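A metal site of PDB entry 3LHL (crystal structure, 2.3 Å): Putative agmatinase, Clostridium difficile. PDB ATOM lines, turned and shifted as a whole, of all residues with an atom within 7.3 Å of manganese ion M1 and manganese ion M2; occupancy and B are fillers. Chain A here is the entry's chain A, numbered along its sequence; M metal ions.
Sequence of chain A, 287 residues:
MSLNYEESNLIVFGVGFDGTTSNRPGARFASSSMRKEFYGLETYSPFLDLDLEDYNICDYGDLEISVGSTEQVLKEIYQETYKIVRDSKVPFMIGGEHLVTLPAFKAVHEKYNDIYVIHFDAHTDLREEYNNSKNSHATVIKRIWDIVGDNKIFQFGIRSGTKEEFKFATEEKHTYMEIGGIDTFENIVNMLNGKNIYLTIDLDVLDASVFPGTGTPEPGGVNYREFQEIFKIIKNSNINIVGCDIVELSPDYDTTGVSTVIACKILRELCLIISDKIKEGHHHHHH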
ATOM      1  N   GLU A  97     -23.083  24.826 -27.273  1.00  0.00           N
ATOM      2  CA  GLU A  97     -22.074  25.737 -26.744  1.00  0.00           C
ATOM      3  C   GLU A  97     -21.115  25.094 -25.737  1.00  0.00           C
ATOM      4  O   GLU A  97     -21.395  24.053 -25.145  1.00  0.00           O
ATOM      5  CB  GLU A  97     -22.725  26.967 -26.118  1.00  0.00           C
ATOM      6  CG  GLU A  97     -23.555  26.696 -24.910  1.00  0.00           C
ATOM      7  CD  GLU A  97     -24.080  27.977 -24.299  1.00  0.00           C
ATOM      8  OE1 GLU A  97     -24.867  28.683 -24.980  1.00  0.00           O
ATOM      9  OE2 GLU A  97     -23.698  28.283 -23.150  1.00  0.00           O
ATOM     10  N   HIS A  98     -19.973  25.756 -25.558  1.00  0.00           N
ATOM     11  CA  HIS A  98     -18.928  25.241 -24.680  1.00  0.00           C
ATOM     12  C   HIS A  98     -19.292  25.170 -23.195  1.00  0.00           C
ATOM     13  O   HIS A  98     -18.638  24.482 -22.424  1.00  0.00           O
ATOM     14  CB  HIS A  98     -17.659  26.056 -24.874  1.00  0.00           C
ATOM     15  CG  HIS A  98     -16.399  25.259 -24.740  1.00  0.00           C
ATOM     16  ND1 HIS A  98     -15.170  25.711 -25.177  1.00  0.00           N
ATOM     17  CD2 HIS A  98     -16.184  24.032 -24.202  1.00  0.00           C
ATOM     18  CE1 HIS A  98     -14.251  24.794 -24.925  1.00  0.00           C
ATOM     19  NE2 HIS A  98     -14.837  23.767 -24.338  1.00  0.00           N
ATOM     20  N   LEU A  99     -20.341  25.872 -22.784  1.00  0.00           N
ATOM     21  CA  LEU A  99     -20.696  25.843 -21.368  1.00  0.00           C
ATOM     22  C   LEU A  99     -21.087  24.440 -20.883  1.00  0.00           C
ATOM     23  O   LEU A  99     -20.879  24.120 -19.712  1.00  0.00           O
ATOM     24  CB  LEU A  99     -21.833  26.833 -21.079  1.00  0.00           C
ATOM     25  CG  LEU A  99     -22.228  27.002 -19.605  1.00  0.00           C
ATOM     26  CD1 LEU A  99     -21.019  27.402 -18.765  1.00  0.00           C
ATOM     27  CD2 LEU A  99     -23.327  28.041 -19.504  1.00  0.00           C
ATOM     28  N   HIS A 119      -7.392  21.389 -23.445  1.00  0.00           N
ATOM     29  CA  HIS A 119      -8.316  22.313 -24.082  1.00  0.00           C
ATOM     30  C   HIS A 119      -7.905  22.826 -25.475  1.00  0.00           C
ATOM     31  O   HIS A 119      -6.880  23.495 -25.614  1.00  0.00           O
ATOM     32  CB  HIS A 119      -8.515  23.481 -23.109  1.00  0.00           C
ATOM     33  CG  HIS A 119      -9.323  24.633 -23.643  1.00  0.00           C
ATOM     34  ND1 HIS A 119     -10.605  24.478 -24.129  1.00  0.00           N
ATOM     35  CD2 HIS A 119      -9.055  25.951 -23.690  1.00  0.00           C
ATOM     36  CE1 HIS A 119     -11.086  25.669 -24.447  1.00  0.00           C
ATOM     37  NE2 HIS A 119     -10.172  26.579 -24.196  1.00  0.00           N
ATOM     38  N   PHE A 120      -8.701  22.505 -26.488  1.00  0.00           N
ATOM     39  CA  PHE A 120      -8.450  22.957 -27.861  1.00  0.00           C
ATOM     40  C   PHE A 120      -9.498  24.019 -28.153  1.00  0.00           C
ATOM     41  O   PHE A 120     -10.696  23.806 -27.946  1.00  0.00           O
ATOM     42  CB  PHE A 120      -8.569  21.792 -28.844  1.00  0.00           C
ATOM     43  CG  PHE A 120      -7.361  20.890 -28.858  1.00  0.00           C
ATOM     44  CD1 PHE A 120      -6.243  21.224 -29.622  1.00  0.00           C
ATOM     45  CD2 PHE A 120      -7.329  19.739 -28.091  1.00  0.00           C
ATOM     46  CE1 PHE A 120      -5.102  20.414 -29.611  1.00  0.00           C
ATOM     47  CE2 PHE A 120      -6.190  18.921 -28.076  1.00  0.00           C
ATOM     48  CZ  PHE A 120      -5.082  19.262 -28.832  1.00  0.00           C
ATOM     49  N   ASP A 121      -9.056  25.162 -28.649  1.00  0.00           N
ATOM     50  CA  ASP A 121      -9.992  26.262 -28.880  1.00  0.00           C
ATOM     51  C   ASP A 121      -9.307  27.403 -29.634  1.00  0.00           C
ATOM     52  O   ASP A 121      -8.075  27.506 -29.661  1.00  0.00           O
ATOM     53  CB  ASP A 121     -10.449  26.801 -27.516  1.00  0.00           C
ATOM     54  CG  ASP A 121     -11.857  27.365 -27.531  1.00  0.00           C
ATOM     55  OD1 ASP A 121     -12.162  28.246 -28.369  1.00  0.00           O
ATOM     56  OD2 ASP A 121     -12.670  26.919 -26.684  1.00  0.00           O
ATOM     57  N   ALA A 122     -10.113  28.258 -30.250  1.00  0.00           N
ATOM     58  CA  ALA A 122      -9.597  29.418 -30.951  1.00  0.00           C
ATOM     59  C   ALA A 122      -9.607  30.544 -29.914  1.00  0.00           C
ATOM     60  O   ALA A 122      -8.853  31.518 -30.028  1.00  0.00           O
ATOM     61  CB  ALA A 122     -10.499  29.781 -32.107  1.00  0.00           C
ATOM     62  N   HIS A 123     -10.451  30.368 -28.900  1.00  0.00           N
ATOM     63  CA  HIS A 123     -10.601  31.341 -27.825  1.00  0.00           C
ATOM     64  C   HIS A 123     -10.109  30.831 -26.469  1.00  0.00           C
ATOM     65  O   HIS A 123     -10.192  29.635 -26.175  1.00  0.00           O
ATOM     66  CB  HIS A 123     -12.068  31.759 -27.711  1.00  0.00           C
ATOM     67  CG  HIS A 123     -12.704  32.050 -29.026  1.00  0.00           C
ATOM     68  ND1 HIS A 123     -13.300  31.073 -29.795  1.00  0.00           N
ATOM     69  CD2 HIS A 123     -12.764  33.194 -29.755  1.00  0.00           C
ATOM     70  CE1 HIS A 123     -13.695  31.599 -30.950  1.00  0.00           C
ATOM     71  NE2 HIS A 123     -13.378  32.881 -30.953  1.00  0.00           N
ATOM     72  N   THR A 124      -9.625  31.756 -25.638  1.00  0.00           N
ATOM     73  CA  THR A 124      -9.122  31.426 -24.315  1.00  0.00           C
ATOM     74  C   THR A 124     -10.232  30.951 -23.378  1.00  0.00           C
ATOM     75  O   THR A 124     -10.054  30.012 -22.603  1.00  0.00           O
ATOM     76  CB  THR A 124      -8.430  32.652 -23.642  1.00  0.00           C
ATOM     77  OG1 THR A 124      -9.420  33.615 -23.264  1.00  0.00           O
ATOM     78  CG2 THR A 124      -7.415  33.298 -24.598  1.00  0.00           C
ATOM     79  N   ASP A 125     -11.395  31.611 -23.454  1.00  0.00           N
ATOM     80  CA  ASP A 125     -12.518  31.278 -22.587  1.00  0.00           C
ATOM     81  C   ASP A 125     -12.144  31.521 -21.113  1.00  0.00           C
ATOM     82  O   ASP A 125     -12.709  30.914 -20.213  1.00  0.00           O
ATOM     83  CB  ASP A 125     -12.928  29.811 -22.769  1.00  0.00           C
ATOM     84  CG  ASP A 125     -13.706  29.588 -24.058  1.00  0.00           C
ATOM     85  OD1 ASP A 125     -14.064  30.589 -24.712  1.00  0.00           O
ATOM     86  OD2 ASP A 125     -13.949  28.417 -24.406  1.00  0.00           O
ATOM     87  N   HIS A 137     -20.328  30.404 -22.460  1.00  0.00           N
ATOM     88  CA  HIS A 137     -19.425  29.580 -23.243  1.00  0.00           C
ATOM     89  C   HIS A 137     -18.034  30.217 -23.251  1.00  0.00           C
ATOM     90  O   HIS A 137     -17.020  29.533 -23.397  1.00  0.00           O
ATOM     91  CB  HIS A 137     -19.924  29.442 -24.700  1.00  0.00           C
ATOM     92  CG  HIS A 137     -20.163  30.745 -25.387  1.00  0.00           C
ATOM     93  ND1 HIS A 137     -21.354  31.437 -25.297  1.00  0.00           N
ATOM     94  CD2 HIS A 137     -19.376  31.486 -26.209  1.00  0.00           C
ATOM     95  CE1 HIS A 137     -21.290  32.537 -26.021  1.00  0.00           C
ATOM     96  NE2 HIS A 137     -20.093  32.593 -26.587  1.00  0.00           N
ATOM     97  N   ALA A 138     -17.996  31.540 -23.053  1.00  0.00           N
ATOM     98  CA  ALA A 138     -16.745  32.303 -23.056  1.00  0.00           C
ATOM     99  C   ALA A 138     -15.993  32.378 -21.729  1.00  0.00           C
ATOM    100  O   ALA A 138     -14.912  32.974 -21.652  1.00  0.00           O
ATOM    101  CB  ALA A 138     -17.018  33.718 -23.566  1.00  0.00           C
ATOM    102  N   VAL A 140     -16.078  29.394 -19.634  1.00  0.00           N
ATOM    103  CA  VAL A 140     -15.982  28.010 -19.204  1.00  0.00           C
ATOM    104  C   VAL A 140     -14.634  27.570 -18.604  1.00  0.00           C
ATOM    105  O   VAL A 140     -14.611  26.904 -17.574  1.00  0.00           O
ATOM    106  CB  VAL A 140     -16.391  27.029 -20.346  1.00  0.00           C
ATOM    107  CG1 VAL A 140     -15.343  27.029 -21.462  1.00  0.00           C
ATOM    108  CG2 VAL A 140     -16.587  25.630 -19.777  1.00  0.00           C
ATOM    109  N   ILE A 141     -13.526  27.949 -19.232  1.00  0.00           N
ATOM    110  CA  ILE A 141     -12.235  27.537 -18.696  1.00  0.00           C
ATOM    111  C   ILE A 141     -11.897  28.243 -17.385  1.00  0.00           C
ATOM    112  O   ILE A 141     -11.220  27.682 -16.526  1.00  0.00           O
ATOM    113  CB  ILE A 141     -11.098  27.773 -19.726  1.00  0.00           C
ATOM    114  CG1 ILE A 141     -11.385  26.948 -20.990  1.00  0.00           C
ATOM    115  CG2 ILE A 141      -9.745  27.345 -19.144  1.00  0.00           C
ATOM    116  CD1 ILE A 141     -11.564  25.470 -20.720  1.00  0.00           C
ATOM    117  N   THR A 200     -11.532  18.468 -23.741  1.00  0.00           N
ATOM    118  CA  THR A 200     -12.590  19.321 -24.260  1.00  0.00           C
ATOM    119  C   THR A 200     -12.111  19.998 -25.537  1.00  0.00           C
ATOM    120  O   THR A 200     -11.156  20.779 -25.535  1.00  0.00           O
ATOM    121  CB  THR A 200     -13.032  20.400 -23.230  1.00  0.00           C
ATOM    122  OG1 THR A 200     -14.042  21.231 -23.827  1.00  0.00           O
ATOM    123  CG2 THR A 200     -11.846  21.256 -22.792  1.00  0.00           C
ATOM    124  N   ILE A 201     -12.789  19.689 -26.635  1.00  0.00           N
ATOM    125  CA  ILE A 201     -12.436  20.237 -27.933  1.00  0.00           C
ATOM    126  C   ILE A 201     -13.475  21.193 -28.511  1.00  0.00           C
ATOM    127  O   ILE A 201     -14.569  20.764 -28.904  1.00  0.00           O
ATOM    128  CB  ILE A 201     -12.191  19.107 -28.962  1.00  0.00           C
ATOM    129  CG1 ILE A 201     -10.917  18.344 -28.593  1.00  0.00           C
ATOM    130  CG2 ILE A 201     -12.105  19.675 -30.383  1.00  0.00           C
ATOM    131  CD1 ILE A 201     -10.610  17.183 -29.521  1.00  0.00           C
ATOM    132  N   ASP A 202     -13.143  22.481 -28.539  1.00  0.00           N
ATOM    133  CA  ASP A 202     -14.027  23.471 -29.144  1.00  0.00           C
ATOM    134  C   ASP A 202     -13.647  23.374 -30.624  1.00  0.00           C
ATOM    135  O   ASP A 202     -12.510  23.685 -30.981  1.00  0.00           O
ATOM    136  CB  ASP A 202     -13.731  24.867 -28.624  1.00  0.00           C
ATOM    137  CG  ASP A 202     -14.632  25.921 -29.230  1.00  0.00           C
ATOM    138  OD1 ASP A 202     -14.886  25.837 -30.447  1.00  0.00           O
ATOM    139  OD2 ASP A 202     -15.078  26.820 -28.501  1.00  0.00           O
ATOM    140  N   LEU A 203     -14.566  22.926 -31.464  1.00  0.00           N
ATOM    141  CA  LEU A 203     -14.272  22.758 -32.883  1.00  0.00           C
ATOM    142  C   LEU A 203     -13.802  24.019 -33.619  1.00  0.00           C
ATOM    143  O   LEU A 203     -13.216  23.904 -34.692  1.00  0.00           O
ATOM    144  CB  LEU A 203     -15.462  22.135 -33.605  1.00  0.00           C
ATOM    145  CG  LEU A 203     -15.835  20.720 -33.112  1.00  0.00           C
ATOM    146  CD1 LEU A 203     -17.148  20.278 -33.723  1.00  0.00           C
ATOM    147  CD2 LEU A 203     -14.717  19.744 -33.468  1.00  0.00           C
ATOM    148  N   ASP A 204     -14.048  25.211 -33.065  1.00  0.00           N
ATOM    149  CA  ASP A 204     -13.578  26.395 -33.769  1.00  0.00           C
ATOM    150  C   ASP A 204     -12.058  26.543 -33.653  1.00  0.00           C
ATOM    151  O   ASP A 204     -11.500  27.560 -34.063  1.00  0.00           O
ATOM    152  CB  ASP A 204     -14.270  27.679 -33.279  1.00  0.00           C
ATOM    153  CG  ASP A 204     -13.949  28.046 -31.843  1.00  0.00           C
ATOM    154  OD1 ASP A 204     -12.858  27.684 -31.342  1.00  0.00           O
ATOM    155  OD2 ASP A 204     -14.790  28.704 -31.217  1.00  0.00           O
ATOM    156  N   VAL A 205     -11.397  25.543 -33.095  1.00  0.00           N
ATOM    157  CA  VAL A 205      -9.946  25.585 -33.013  1.00  0.00           C
ATOM    158  C   VAL A 205      -9.460  25.481 -34.452  1.00  0.00           C
ATOM    159  O   VAL A 205      -8.383  25.956 -34.801  1.00  0.00           O
ATOM    160  CB  VAL A 205      -9.371  24.409 -32.182  1.00  0.00           C
ATOM    161  CG1 VAL A 205      -9.595  23.072 -32.896  1.00  0.00           C
ATOM    162  CG2 VAL A 205      -7.886  24.634 -31.927  1.00  0.00           C
ATOM    163  N   THR A 214     -19.639  27.468 -37.175  1.00  0.00           N
ATOM    164  CA  THR A 214     -19.422  27.669 -35.750  1.00  0.00           C
ATOM    165  C   THR A 214     -19.834  29.081 -35.373  1.00  0.00           C
ATOM    166  O   THR A 214     -19.930  29.958 -36.238  1.00  0.00           O
ATOM    167  CB  THR A 214     -17.942  27.406 -35.376  1.00  0.00           C
ATOM    168  OG1 THR A 214     -17.822  27.294 -33.946  1.00  0.00           O
ATOM    169  CG2 THR A 214     -17.059  28.553 -35.851  1.00  0.00           C
ATOM    170  N   THR A 216     -18.305  31.627 -33.475  1.00  0.00           N
ATOM    171  CA  THR A 216     -17.337  32.717 -33.546  1.00  0.00           C
ATOM    172  C   THR A 216     -16.089  32.314 -34.332  1.00  0.00           C
ATOM    173  O   THR A 216     -15.033  32.086 -33.758  1.00  0.00           O
ATOM    174  CB  THR A 216     -16.894  33.113 -32.124  1.00  0.00           C
ATOM    175  OG1 THR A 216     -18.026  33.074 -31.265  1.00  0.00           O
ATOM    176  CG2 THR A 216     -16.275  34.515 -32.118  1.00  0.00           C
ATOM    177  N   VAL A 247     -17.414  20.562 -29.057  1.00  0.00           N
ATOM    178  CA  VAL A 247     -18.479  21.546 -28.994  1.00  0.00           C
ATOM    179  C   VAL A 247     -18.368  22.670 -30.007  1.00  0.00           C
ATOM    180  O   VAL A 247     -17.375  22.786 -30.717  1.00  0.00           O
ATOM    181  CB  VAL A 247     -18.521  22.187 -27.574  1.00  0.00           C
ATOM    182  CG1 VAL A 247     -18.781  21.124 -26.508  1.00  0.00           C
ATOM    183  CG2 VAL A 247     -17.200  22.892 -27.288  1.00  0.00           C
ATOM    184  N   GLU A 248     -19.421  23.487 -30.043  1.00  0.00           N
ATOM    185  CA  GLU A 248     -19.508  24.665 -30.896  1.00  0.00           C
ATOM    186  C   GLU A 248     -19.767  24.460 -32.389  1.00  0.00           C
ATOM    187  O   GLU A 248     -19.613  25.396 -33.189  1.00  0.00           O
ATOM    188  CB  GLU A 248     -18.272  25.560 -30.675  1.00  0.00           C
ATOM    189  CG  GLU A 248     -18.200  26.152 -29.260  1.00  0.00           C
ATOM    190  CD  GLU A 248     -19.415  27.021 -28.891  1.00  0.00           C
ATOM    191  OE1 GLU A 248     -20.445  26.937 -29.585  1.00  0.00           O
ATOM    192  OE2 GLU A 248     -19.340  27.779 -27.894  1.00  0.00           O
HETATM  193 MN    MN M   1     -14.190  28.873 -29.279  1.00  0.00          MN
HETATM  194 MN    MN M   2     -14.743  27.504 -26.417  1.00  0.00          MN
HETATM  195 MN    MN M   3     -16.512  29.593 -27.249  1.00  0.00          MN
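Four residues have an atom within 4 Å of manganese ion M1: Asp 121, His 123, Asp 202 and Asp 204.
Manganese ion M1 is bound by the side-chain carboxylate of Asp 204, the side-chain carboxylate of Asp 121, the side-chain carboxylate of Asp 202 and a ring nitrogen (ND1) of His 123.
Slightly farther from manganese ion M1 lies OD1 of Asp 204 (2.7 Å).
Four residues have an atom within 4 Å of manganese ion M2: His 98, Asp 121, Asp 125 and Asp 202.
The nearest printed residue that does not touch manganese ion M2 is His 137 (4.3 Å).
The backbone carbonyl oxygen (O) of Asp 125 lies within hydrogen-bond range of the backbone NH (N) of Ile 141 (3.2 Å).
OD1 of Asp 204 lies within hydrogen-bond range of N of Ala 122 (3.0 Å).
O of Phe 120 sits at hydrogen-bond distance from N of Asp 202, 2.8 Å away.
A ring nitrogen (NE2) of His 98 lies within hydrogen-bond range of the side-chain hydroxyl of Thr 200 (2.7 Å).
OE2 of Glu 248 is in hydrogen-bond range of N of His 98, 3.2 Å away.
NE2 of His 123 sits close to O of Thr 216, at 3.4 Å.
Manganese ion M2 is bound by OD2 of Asp 121 (2.2 Å), OD2 of Asp 202 (2.2 Å), ND1 of His 98 (2.2 Å) and OD2 of Asp 125 (2.3 Å).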
